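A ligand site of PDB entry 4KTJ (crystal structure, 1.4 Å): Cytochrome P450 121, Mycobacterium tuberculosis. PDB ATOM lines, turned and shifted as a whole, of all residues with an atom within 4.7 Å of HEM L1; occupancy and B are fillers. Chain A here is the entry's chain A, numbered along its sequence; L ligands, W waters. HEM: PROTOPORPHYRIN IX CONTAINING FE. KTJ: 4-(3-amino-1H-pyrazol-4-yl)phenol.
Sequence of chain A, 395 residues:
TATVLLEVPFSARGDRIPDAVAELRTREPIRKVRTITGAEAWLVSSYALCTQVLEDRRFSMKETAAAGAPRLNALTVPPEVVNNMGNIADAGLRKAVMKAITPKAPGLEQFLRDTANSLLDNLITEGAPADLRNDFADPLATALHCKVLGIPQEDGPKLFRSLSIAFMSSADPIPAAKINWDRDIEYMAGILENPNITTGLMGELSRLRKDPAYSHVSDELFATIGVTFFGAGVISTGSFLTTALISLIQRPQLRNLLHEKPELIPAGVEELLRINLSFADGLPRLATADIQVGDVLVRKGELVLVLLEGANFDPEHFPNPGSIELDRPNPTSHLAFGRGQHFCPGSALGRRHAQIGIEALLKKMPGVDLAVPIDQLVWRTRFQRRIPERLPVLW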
ATOM      1  N   MET A  61       1.803  21.536   6.748  1.00  0.00           N
ATOM      2  CA  MET A  61       0.874  21.247   7.861  1.00  0.00           C
ATOM      3  C   MET A  61       0.501  19.797   7.777  1.00  0.00           C
ATOM      4  O   MET A  61       0.538  19.058   8.807  1.00  0.00           O
ATOM      5  CB  MET A  61      -0.490  22.070   7.858  1.00  0.00           C
ATOM      6  CG  MET A  61      -1.726  21.375   8.865  1.00  0.00           C
ATOM      7  SD  MET A  61      -3.118  22.525   8.526  1.00  0.00           S
ATOM      8  CE  MET A  61      -2.492  24.038   9.204  1.00  0.00           C
ATOM      9  N   ASN A  84      -7.736  19.012   6.944  1.00  0.00           N
ATOM     10  CA  ASN A  84      -9.163  19.243   6.843  1.00  0.00           C
ATOM     11  C   ASN A  84      -9.444  20.186   5.695  1.00  0.00           C
ATOM     12  O   ASN A  84     -10.246  19.873   4.811  1.00  0.00           O
ATOM     13  CB  ASN A  84      -9.627  19.761   8.154  1.00  0.00           C
ATOM     14  CG  ASN A  84     -11.121  19.889   8.299  1.00  0.00           C
ATOM     15  OD1 ASN A  84     -11.887  19.065   7.822  1.00  0.00           O
ATOM     16  ND2 ASN A  84     -11.532  20.977   8.959  1.00  0.00           N
ATOM     17  N   MET A  85      -8.773  21.309   5.582  1.00  0.00           N
ATOM     18  CA  MET A  85      -9.031  22.208   4.436  1.00  0.00           C
ATOM     19  C   MET A  85      -8.630  21.666   3.071  1.00  0.00           C
ATOM     20  O   MET A  85      -9.321  21.878   2.082  1.00  0.00           O
ATOM     21  CB  MET A  85      -8.360  23.574   4.699  1.00  0.00           C
ATOM     22  CG  MET A  85      -9.121  24.451   5.680  1.00  0.00           C
ATOM     23  SD  MET A  85     -10.825  24.963   5.334  1.00  0.00           S
ATOM     24  CE  MET A  85     -10.876  25.117   3.533  1.00  0.00           C
ATOM     25  N   ILE A 101     -19.724  30.949   6.177  1.00  0.00           N
ATOM     26  CA  ILE A 101     -19.222  31.359   7.503  1.00  0.00           C
ATOM     27  C   ILE A 101     -18.833  32.847   7.513  1.00  0.00           C
ATOM     28  O   ILE A 101     -18.098  33.287   8.383  1.00  0.00           O
ATOM     29  CB  ILE A 101     -18.081  30.447   7.975  1.00  0.00           C
ATOM     30  CG1 ILE A 101     -16.875  30.613   7.101  1.00  0.00           C
ATOM     31  CG2 ILE A 101     -18.540  28.995   8.058  1.00  0.00           C
ATOM     32  CD1 ILE A 101     -15.655  29.887   7.565  1.00  0.00           C
ATOM     33  N   HIS A 145     -21.929  30.226  16.601  1.00  0.00           N
ATOM     34  CA  HIS A 145     -21.617  29.063  15.767  1.00  0.00           C
ATOM     35  C   HIS A 145     -22.773  28.150  15.604  1.00  0.00           C
ATOM     36  O   HIS A 145     -22.890  27.552  14.494  1.00  0.00           O
ATOM     37  CB  HIS A 145     -20.317  28.380  16.256  1.00  0.00           C
ATOM     38  CG  HIS A 145     -19.108  29.162  15.949  1.00  0.00           C
ATOM     39  ND1 HIS A 145     -18.698  30.297  16.670  1.00  0.00           N
ATOM     40  CD2 HIS A 145     -18.246  29.141  14.876  1.00  0.00           C
ATOM     41  CE1 HIS A 145     -17.654  30.878  16.117  1.00  0.00           C
ATOM     42  NE2 HIS A 145     -17.367  30.204  14.991  1.00  0.00           N
ATOM     43  N   PHE A 229     -15.483  22.911  12.182  1.00  0.00           N
ATOM     44  CA  PHE A 229     -15.799  24.371  12.089  1.00  0.00           C
ATOM     45  C   PHE A 229     -16.448  24.812  13.393  1.00  0.00           C
ATOM     46  O   PHE A 229     -16.102  25.922  13.912  1.00  0.00           O
ATOM     47  CB  PHE A 229     -16.555  24.722  10.752  1.00  0.00           C
ATOM     48  CG  PHE A 229     -15.597  24.916   9.620  1.00  0.00           C
ATOM     49  CD1 PHE A 229     -14.890  23.848   9.113  1.00  0.00           C
ATOM     50  CD2 PHE A 229     -15.290  26.181   9.065  1.00  0.00           C
ATOM     51  CE1 PHE A 229     -13.986  24.053   8.085  1.00  0.00           C
ATOM     52  CE2 PHE A 229     -14.329  26.346   8.080  1.00  0.00           C
ATOM     53  CZ  PHE A 229     -13.727  25.331   7.582  1.00  0.00           C
ATOM     54  N   ALA A 232     -13.247  24.663  16.067  1.00  0.00           N
ATOM     55  CA  ALA A 232     -12.228  25.683  15.860  1.00  0.00           C
ATOM     56  C   ALA A 232     -12.819  27.084  16.016  1.00  0.00           C
ATOM     57  O   ALA A 232     -12.132  27.934  16.648  1.00  0.00           O
ATOM     58  CB  ALA A 232     -11.640  25.530  14.453  1.00  0.00           C
ATOM     59  N   GLY A 233     -13.994  27.338  15.467  1.00  0.00           N
ATOM     60  CA  GLY A 233     -14.581  28.645  15.559  1.00  0.00           C
ATOM     61  C   GLY A 233     -14.896  28.996  17.039  1.00  0.00           C
ATOM     62  O   GLY A 233     -14.549  30.119  17.438  1.00  0.00           O
ATOM     63  N   SER A 236     -11.715  29.429  19.216  1.00  0.00           N
ATOM     64  CA  SER A 236     -10.869  30.517  18.793  1.00  0.00           C
ATOM     65  C   SER A 236     -11.512  31.872  19.077  1.00  0.00           C
ATOM     66  O   SER A 236     -10.847  32.766  19.640  1.00  0.00           O
ATOM     67  CB  SER A 236     -10.521  30.441  17.300  1.00  0.00           C
ATOM     68  OG  SER A 236      -9.794  29.205  17.068  1.00  0.00           O
ATOM     69  N   THR A 237     -12.772  32.048  18.831  1.00  0.00           N
ATOM     70  CA  THR A 237     -13.456  33.292  19.102  1.00  0.00           C
ATOM     71  C   THR A 237     -13.707  33.459  20.606  1.00  0.00           C
ATOM     72  O   THR A 237     -13.548  34.602  21.099  1.00  0.00           O
ATOM     73  CB  THR A 237     -14.761  33.390  18.340  1.00  0.00           C
ATOM     74  OG1 THR A 237     -15.653  32.337  18.672  1.00  0.00           O
ATOM     75  CG2 THR A 237     -14.560  33.466  16.842  1.00  0.00           C
ATOM     76  N   PHE A 240     -10.111  34.260  22.074  1.00  0.00           N
ATOM     77  CA  PHE A 240      -9.712  35.596  21.696  1.00  0.00           C
ATOM     78  C   PHE A 240     -10.534  36.686  22.384  1.00  0.00           C
ATOM     79  O   PHE A 240      -9.889  37.598  22.983  1.00  0.00           O
ATOM     80  CB  PHE A 240      -9.732  35.809  20.156  1.00  0.00           C
ATOM     81  CG  PHE A 240      -9.476  37.200  19.819  1.00  0.00           C
ATOM     82  CD1 PHE A 240      -8.254  37.772  20.093  1.00  0.00           C
ATOM     83  CD2 PHE A 240     -10.413  38.037  19.251  1.00  0.00           C
ATOM     84  CE1 PHE A 240      -8.008  39.099  19.880  1.00  0.00           C
ATOM     85  CE2 PHE A 240     -10.170  39.384  19.060  1.00  0.00           C
ATOM     86  CZ  PHE A 240      -8.984  39.902  19.391  1.00  0.00           C
ATOM     87  N   LEU A 273      -6.140  41.946  18.172  1.00  0.00           N
ATOM     88  CA  LEU A 273      -5.668  40.727  17.461  1.00  0.00           C
ATOM     89  C   LEU A 273      -4.202  40.711  17.402  1.00  0.00           C
ATOM     90  O   LEU A 273      -3.533  39.686  17.675  1.00  0.00           O
ATOM     91  CB  LEU A 273      -6.255  40.670  16.052  1.00  0.00           C
ATOM     92  CG  LEU A 273      -7.702  40.303  15.972  1.00  0.00           C
ATOM     93  CD1 LEU A 273      -8.381  40.752  14.704  1.00  0.00           C
ATOM     94  CD2 LEU A 273      -7.918  38.744  16.140  1.00  0.00           C
ATOM     95  N   PHE A 279      -3.027  31.822  21.160  1.00  0.00           N
ATOM     96  CA  PHE A 279      -2.383  30.557  20.768  1.00  0.00           C
ATOM     97  C   PHE A 279      -1.277  30.230  21.710  1.00  0.00           C
ATOM     98  O   PHE A 279      -0.302  30.914  21.825  1.00  0.00           O
ATOM     99  CB  PHE A 279      -1.916  30.628  19.294  1.00  0.00           C
ATOM    100  CG  PHE A 279      -3.014  30.332  18.277  1.00  0.00           C
ATOM    101  CD1 PHE A 279      -4.120  31.055  18.126  1.00  0.00           C
ATOM    102  CD2 PHE A 279      -2.892  29.175  17.441  1.00  0.00           C
ATOM    103  CE1 PHE A 279      -5.132  30.735  17.195  1.00  0.00           C
ATOM    104  CE2 PHE A 279      -3.931  28.832  16.608  1.00  0.00           C
ATOM    105  CZ  PHE A 279      -5.010  29.591  16.455  1.00  0.00           C
ATOM    106  N   LEU A 283       2.655  27.493  15.632  1.00  0.00           N
ATOM    107  CA  LEU A 283       1.937  26.729  14.637  1.00  0.00           C
ATOM    108  C   LEU A 283       2.929  25.709  14.042  1.00  0.00           C
ATOM    109  O   LEU A 283       4.037  26.037  13.657  1.00  0.00           O
ATOM    110  CB  LEU A 283       1.479  27.613  13.426  1.00  0.00           C
ATOM    111  CG  LEU A 283       0.557  28.800  13.771  1.00  0.00           C
ATOM    112  CD1 LEU A 283       0.171  29.497  12.494  1.00  0.00           C
ATOM    113  CD2 LEU A 283      -0.680  28.316  14.563  1.00  0.00           C
ATOM    114  N   ARG A 285       4.646  22.819  11.613  1.00  0.00           N
ATOM    115  CA  ARG A 285       4.928  22.478  10.187  1.00  0.00           C
ATOM    116  C   ARG A 285       6.027  21.371  10.155  1.00  0.00           C
ATOM    117  O   ARG A 285       6.929  21.434  11.033  1.00  0.00           O
ATOM    118  CB  ARG A 285       5.399  23.697   9.385  1.00  0.00           C
ATOM    119  CG  ARG A 285       4.378  24.821   9.290  1.00  0.00           C
ATOM    120  CD  ARG A 285       3.199  24.396   8.472  1.00  0.00           C
ATOM    121  NE  ARG A 285       2.283  25.582   8.187  1.00  0.00           N
ATOM    122  CZ  ARG A 285       1.208  25.872   8.872  1.00  0.00           C
ATOM    123  NH1 ARG A 285       0.911  25.345  10.061  1.00  0.00           N
ATOM    124  NH2 ARG A 285       0.433  26.922   8.416  1.00  0.00           N
ATOM    125  N   LEU A 308       3.530  32.914  16.849  1.00  0.00           N
ATOM    126  CA  LEU A 308       2.734  34.051  16.352  1.00  0.00           C
ATOM    127  C   LEU A 308       3.117  35.317  17.046  1.00  0.00           C
ATOM    128  O   LEU A 308       3.234  36.427  16.458  1.00  0.00           O
ATOM    129  CB  LEU A 308       1.257  33.808  16.372  1.00  0.00           C
ATOM    130  CG  LEU A 308       0.805  32.638  15.503  1.00  0.00           C
ATOM    131  CD1 LEU A 308      -0.731  32.540  15.602  1.00  0.00           C
ATOM    132  CD2 LEU A 308       1.299  32.780  14.077  1.00  0.00           C
ATOM    133  N   LEU A 335      -0.003  38.399  12.123  1.00  0.00           N
ATOM    134  CA  LEU A 335      -0.133  36.939  11.877  1.00  0.00           C
ATOM    135  C   LEU A 335      -1.192  36.330  12.775  1.00  0.00           C
ATOM    136  O   LEU A 335      -1.181  35.091  12.914  1.00  0.00           O
ATOM    137  CB  LEU A 335       1.196  36.257  11.951  1.00  0.00           C
ATOM    138  CG  LEU A 335       2.320  36.756  11.052  1.00  0.00           C
ATOM    139  CD1 LEU A 335       3.517  35.787  11.029  1.00  0.00           C
ATOM    140  CD2 LEU A 335       1.902  37.116   9.694  1.00  0.00           C
ATOM    141  N   ALA A 336      -2.051  37.043  13.378  1.00  0.00           N
ATOM    142  CA  ALA A 336      -3.037  36.459  14.290  1.00  0.00           C
ATOM    143  C   ALA A 336      -3.950  35.417  13.667  1.00  0.00           C
ATOM    144  O   ALA A 336      -4.405  34.494  14.327  1.00  0.00           O
ATOM    145  CB  ALA A 336      -3.958  37.474  14.952  1.00  0.00           C
ATOM    146  N   PHE A 337      -4.162  35.525  12.344  1.00  0.00           N
ATOM    147  CA  PHE A 337      -4.972  34.527  11.533  1.00  0.00           C
ATOM    148  C   PHE A 337      -4.057  33.642  10.727  1.00  0.00           C
ATOM    149  O   PHE A 337      -4.594  32.981   9.769  1.00  0.00           O
ATOM    150  CB  PHE A 337      -5.953  35.301  10.692  1.00  0.00           C
ATOM    151  CG  PHE A 337      -7.015  35.972  11.469  1.00  0.00           C
ATOM    152  CD1 PHE A 337      -7.924  35.258  12.237  1.00  0.00           C
ATOM    153  CD2 PHE A 337      -7.152  37.358  11.384  1.00  0.00           C
ATOM    154  CE1 PHE A 337      -8.932  35.905  12.961  1.00  0.00           C
ATOM    155  CE2 PHE A 337      -8.210  37.939  12.067  1.00  0.00           C
ATOM    156  CZ  PHE A 337      -9.106  37.234  12.816  1.00  0.00           C
ATOM    157  N   GLY A 338      -2.803  33.603  10.985  1.00  0.00           N
ATOM    158  CA  GLY A 338      -1.840  32.890  10.166  1.00  0.00           C
ATOM    159  C   GLY A 338      -1.521  33.651   8.865  1.00  0.00           C
ATOM    160  O   GLY A 338      -1.687  34.927   8.808  1.00  0.00           O
ATOM    161  N   GLN A 341      -1.093  29.395   2.767  1.00  0.00           N
ATOM    162  CA  GLN A 341      -1.997  28.308   2.321  1.00  0.00           C
ATOM    163  C   GLN A 341      -3.111  28.116   3.404  1.00  0.00           C
ATOM    164  O   GLN A 341      -4.252  27.845   3.087  1.00  0.00           O
ATOM    165  CB  GLN A 341      -1.216  26.981   2.149  1.00  0.00           C
ATOM    166  CG  GLN A 341      -2.082  25.851   1.611  1.00  0.00           C
ATOM    167  CD  GLN A 341      -2.738  26.034   0.287  1.00  0.00           C
ATOM    168  OE1 GLN A 341      -3.750  25.318   0.007  1.00  0.00           O
ATOM    169  NE2 GLN A 341      -2.145  26.817  -0.595  1.00  0.00           N
ATOM    170  N   HIS A 342      -2.727  28.168   4.713  1.00  0.00           N
ATOM    171  CA  HIS A 342      -3.635  27.834   5.747  1.00  0.00           C
ATOM    172  C   HIS A 342      -4.223  28.987   6.503  1.00  0.00           C
ATOM    173  O   HIS A 342      -4.698  28.896   7.670  1.00  0.00           O
ATOM    174  CB  HIS A 342      -2.994  26.853   6.692  1.00  0.00           C
ATOM    175  CG  HIS A 342      -2.631  25.558   5.995  1.00  0.00           C
ATOM    176  ND1 HIS A 342      -3.596  24.623   5.701  1.00  0.00           N
ATOM    177  CD2 HIS A 342      -1.440  25.070   5.542  1.00  0.00           C
ATOM    178  CE1 HIS A 342      -3.003  23.598   5.087  1.00  0.00           C
ATOM    179  NE2 HIS A 342      -1.733  23.868   4.936  1.00  0.00           N
ATOM    180  N   PHE A 343      -4.183  30.196   5.898  1.00  0.00           N
ATOM    181  CA  PHE A 343      -4.798  31.405   6.438  1.00  0.00           C
ATOM    182  C   PHE A 343      -6.205  31.118   6.897  1.00  0.00           C
ATOM    183  O   PHE A 343      -7.019  30.419   6.209  1.00  0.00           O
ATOM    184  CB  PHE A 343      -4.784  32.536   5.415  1.00  0.00           C
ATOM    185  CG  PHE A 343      -5.349  33.824   5.944  1.00  0.00           C
ATOM    186  CD1 PHE A 343      -4.534  34.688   6.633  1.00  0.00           C
ATOM    187  CD2 PHE A 343      -6.663  34.155   5.768  1.00  0.00           C
ATOM    188  CE1 PHE A 343      -5.036  35.889   7.154  1.00  0.00           C
ATOM    189  CE2 PHE A 343      -7.192  35.346   6.334  1.00  0.00           C
ATOM    190  CZ  PHE A 343      -6.361  36.185   7.034  1.00  0.00           C
ATOM    191  N   CYS A 344      -6.603  31.543   8.125  1.00  0.00           N
ATOM    192  CA  CYS A 344      -7.847  31.204   8.758  1.00  0.00           C
ATOM    193  C   CYS A 344      -9.071  31.427   7.827  1.00  0.00           C
ATOM    194  O   CYS A 344      -9.262  32.629   7.470  1.00  0.00           O
ATOM    195  CB  CYS A 344      -8.022  32.089  10.020  1.00  0.00           C
ATOM    196  SG  CYS A 344      -9.552  31.800  10.923  1.00  0.00           S
ATOM    197  N   PRO A 345      -9.929  30.517   7.618  1.00  0.00           N
ATOM    198  CA  PRO A 345     -11.104  30.716   6.769  1.00  0.00           C
ATOM    199  C   PRO A 345     -12.171  31.481   7.529  1.00  0.00           C
ATOM    200  O   PRO A 345     -13.098  32.040   6.887  1.00  0.00           O
ATOM    201  CB  PRO A 345     -11.551  29.294   6.463  1.00  0.00           C
ATOM    202  CG  PRO A 345     -11.164  28.493   7.618  1.00  0.00           C
ATOM    203  CD  PRO A 345      -9.807  29.083   7.946  1.00  0.00           C
ATOM    204  N   GLY A 346     -12.105  31.594   8.850  1.00  0.00           N
ATOM    205  CA  GLY A 346     -13.129  32.340   9.605  1.00  0.00           C
ATOM    206  C   GLY A 346     -12.701  33.744  10.074  1.00  0.00           C
ATOM    207  O   GLY A 346     -13.371  34.265  10.966  1.00  0.00           O
ATOM    208  N   LEU A 349     -15.492  36.470  10.320  1.00  0.00           N
ATOM    209  CA  LEU A 349     -16.363  36.083  11.353  1.00  0.00           C
ATOM    210  C   LEU A 349     -15.766  36.377  12.795  1.00  0.00           C
ATOM    211  O   LEU A 349     -16.433  36.904  13.709  1.00  0.00           O
ATOM    212  CB  LEU A 349     -16.867  34.636  11.264  1.00  0.00           C
ATOM    213  CG  LEU A 349     -17.961  34.224  12.143  1.00  0.00           C
ATOM    214  CD1 LEU A 349     -19.275  35.004  11.942  1.00  0.00           C
ATOM    215  CD2 LEU A 349     -18.172  32.725  11.909  1.00  0.00           C
ATOM    216  N   GLY A 350     -14.526  35.987  12.974  1.00  0.00           N
ATOM    217  CA  GLY A 350     -13.801  36.254  14.267  1.00  0.00           C
ATOM    218  C   GLY A 350     -13.710  37.734  14.531  1.00  0.00           C
ATOM    219  O   GLY A 350     -13.944  38.069  15.698  1.00  0.00           O
HETATM  220  CHA HEM L   1      -6.861  28.267  10.996  1.00  0.00           C
HETATM  221  CHB HEM L   1      -6.674  31.870  14.196  1.00  0.00           C
HETATM  222  CHC HEM L   1     -11.520  32.108  14.176  1.00  0.00           C
HETATM  223  CHD HEM L   1     -11.630  28.003  11.555  1.00  0.00           C
HETATM  224  C1A HEM L   1      -6.344  29.320  11.775  1.00  0.00           C
HETATM  225  C2A HEM L   1      -5.012  29.662  11.891  1.00  0.00           C
HETATM  226  C3A HEM L   1      -4.946  30.632  12.877  1.00  0.00           C
HETATM  227  C4A HEM L   1      -6.301  30.871  13.264  1.00  0.00           C
HETATM  228  CMA HEM L   1      -3.721  31.272  13.414  1.00  0.00           C
HETATM  229  CAA HEM L   1      -3.868  29.097  11.137  1.00  0.00           C
HETATM  230  CBA HEM L   1      -3.397  27.695  11.587  1.00  0.00           C
HETATM  231  CGA HEM L   1      -2.158  27.241  10.867  1.00  0.00           C
HETATM  232  O1A HEM L   1      -1.719  27.862   9.868  1.00  0.00           O
HETATM  233  O2A HEM L   1      -1.506  26.235  11.336  1.00  0.00           O
HETATM  234  C1B HEM L   1      -8.027  32.226  14.519  1.00  0.00           C
HETATM  235  C2B HEM L   1      -8.413  33.317  15.408  1.00  0.00           C
HETATM  236  C3B HEM L   1      -9.749  33.355  15.397  1.00  0.00           C
HETATM  237  C4B HEM L   1     -10.229  32.335  14.457  1.00  0.00           C
HETATM  238  CMB HEM L   1      -7.407  34.182  16.187  1.00  0.00           C
HETATM  239  CAB HEM L   1     -10.697  34.286  16.063  1.00  0.00           C
HETATM  240  CBB HEM L   1     -10.345  35.474  16.540  1.00  0.00           C
HETATM  241  C1C HEM L   1     -12.047  31.064  13.414  1.00  0.00           C
HETATM  242  C2C HEM L   1     -13.371  30.776  13.116  1.00  0.00           C
HETATM  243  C3C HEM L   1     -13.400  29.566  12.416  1.00  0.00           C
HETATM  244  C4C HEM L   1     -12.052  29.187  12.222  1.00  0.00           C
HETATM  245  CMC HEM L   1     -14.554  31.624  13.464  1.00  0.00           C
HETATM  246  CAC HEM L   1     -14.556  28.833  11.878  1.00  0.00           C
HETATM  247  CBC HEM L   1     -15.811  29.162  11.994  1.00  0.00           C
HETATM  248  C1D HEM L   1     -10.351  27.660  11.240  1.00  0.00           C
HETATM  249  C2D HEM L   1      -9.955  26.442  10.478  1.00  0.00           C
HETATM  250  C3D HEM L   1      -8.622  26.615  10.260  1.00  0.00           C
HETATM  251  C4D HEM L   1      -8.125  27.813  10.989  1.00  0.00           C
HETATM  252  CMD HEM L   1     -10.964  25.380   9.996  1.00  0.00           C
HETATM  253  CAD HEM L   1      -7.663  25.671   9.540  1.00  0.00           C
HETATM  254  CBD HEM L   1      -7.334  26.207   8.104  1.00  0.00           C
HETATM  255  CGD HEM L   1      -6.341  25.347   7.326  1.00  0.00           C
HETATM  256  O1D HEM L   1      -6.227  25.774   6.137  1.00  0.00           O
HETATM  257  O2D HEM L   1      -5.881  24.354   7.867  1.00  0.00           O
HETATM  258  NA  HEM L   1      -7.156  30.093  12.546  1.00  0.00           N
HETATM  259  NB  HEM L   1      -9.139  31.699  14.003  1.00  0.00           N
HETATM  260  NC  HEM L   1     -11.239  30.124  12.806  1.00  0.00           N
HETATM  261  ND  HEM L   1      -9.246  28.493  11.413  1.00  0.00           N
HETATM  262 FE   HEM L   1      -9.202  30.143  12.624  1.00  0.00          FE
HETATM  263  CAH KTJ L   2     -10.914  21.655  14.210  1.00  0.00           C
HETATM  264  CAI KTJ L   2     -10.465  22.229  13.024  1.00  0.00           C
HETATM  265  CAJ KTJ L   2      -9.437  21.638  12.306  1.00  0.00           C
HETATM  266  OAM KTJ L   2      -9.010  22.206  11.150  1.00  0.00           O
HETATM  267  CAK KTJ L   2      -8.843  20.471  12.777  1.00  0.00           C
HETATM  268  CAL KTJ L   2      -9.292  19.897  13.962  1.00  0.00           C
HETATM  269  CAG KTJ L   2     -10.321  20.488  14.680  1.00  0.00           C
HETATM  270  CAC KTJ L   2     -10.739  19.934  15.811  1.00  0.00           C
HETATM  271  CAB KTJ L   2      -9.999  19.228  16.656  1.00  0.00           C
HETATM  272  NAA KTJ L   2     -10.827  18.873  17.652  1.00  0.00           N
HETATM  273  NAE KTJ L   2     -11.972  19.309  17.443  1.00  0.00           N
HETATM  274  CAD KTJ L   2     -11.973  19.992  16.293  1.00  0.00           C
HETATM  275  NAF KTJ L   2     -13.057  20.588  15.800  1.00  0.00           N
HETATM  276  O   HOH W   1      -1.506  30.089   8.307  1.00  0.00           O
HETATM  277  O   HOH W   2      -5.967  25.430   3.121  1.00  0.00           O
HETATM  278  O   HOH W   3      -6.650  22.098   7.512  1.00  0.00           O
HETATM  279  O   HOH W   4      -2.228  24.649  13.285  1.00  0.00           O
HETATM  280  O   HOH W   5      -7.499  27.883   5.089  1.00  0.00           O
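FE of HEM L1 is bound by SG of Cys 344 (2.4 Å).
O1A of HEM L1 is in salt-bridge range of NH2 of Arg 285.
ND1 of His 342 lies within hydrogen-bond range of O1D of HEM L1, 2.9 Å away.
Water W3 lies within hydrogen-bond range of an oxygen (O2D) of HEM L1 (2.4 Å), the backbone NH of Met 85 (3.0 Å), the backbone NH of Asn 84 (3.3 Å) and the side-chain sulfur of Met 61 (3.7 Å).
Water W5 bridges an oxygen (O1D) of HEM L1 and the backbone carbonyl oxygen of Phe 343.
Water W1 lies within hydrogen-bond range of an oxygen (O1A) of HEM L1 and the backbone carbonyl oxygen (O) of His 342.
Water W2 lies within hydrogen-bond range of the backbone carbonyl oxygen of Gln 341 and an oxygen (O1D) of HEM L1.
The side-chain sulfur (SD) of Met 61 lies close to an oxygen (O2D) of HEM L1 (3.4 Å).
Met 85 touches HEM L1 (CG to O1D, 3.2 Å).
NE2 of His 145 touches CMC of HEM L1, 3.5 Å away.
Phe 229 touches HEM L1 (CZ to CMD, 3.7 Å).
CB of Ala 232 touches CHD of HEM L1, at 3.8 Å.
Gly 233 touches HEM L1 (CA to C2C, 3.5 Å).
CB of Ser 236 touches C4B of HEM L1, 3.4 Å away.
CG2 of Thr 237 touches CMC of HEM L1, at 3.8 Å.
CB of Phe 240 touches CBB of HEM L1, 3.7 Å away.
Phe 279 touches HEM L1 (CE1 to CHB, 3.6 Å).
CD1 of Leu 283 touches O1A of HEM L1, at 3.6 Å.
Leu 308 touches HEM L1.
Ala 336 touches HEM L1.
Phe 337 touches HEM L1.
Gly 338 touches HEM L1 (N to CMA, 3.5 Å).
Pro 345 touches HEM L1 (CD to ND, 3.6 Å).
O of Gly 346 touches CMC of HEM L1, at 3.8 Å.
The nearest printed residue that does not touch HEM L1 is Leu 349 (4.1 Å).
The side-chain hydroxyl (OG) of Ser 236 lies within hydrogen-bond range of the backbone carbonyl oxygen (O) of Ala 232 (2.7 Å).
A ring nitrogen (ND1) of His 342 sits at hydrogen-bond distance from the side-chain sulfur of Met 61 (3.6 Å).
The backbone NH (N) of Gly 346 lies close to the side-chain sulfur (SG) of Cys 344 (3.3 Å).
O of Gly 233 is in hydrogen-bond range of OG1 of Thr 237, 2.8 Å away.
The backbone NH of Cys 344 lies within hydrogen-bond range of the backbone carbonyl oxygen of Phe 337, at 3.0 Å.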
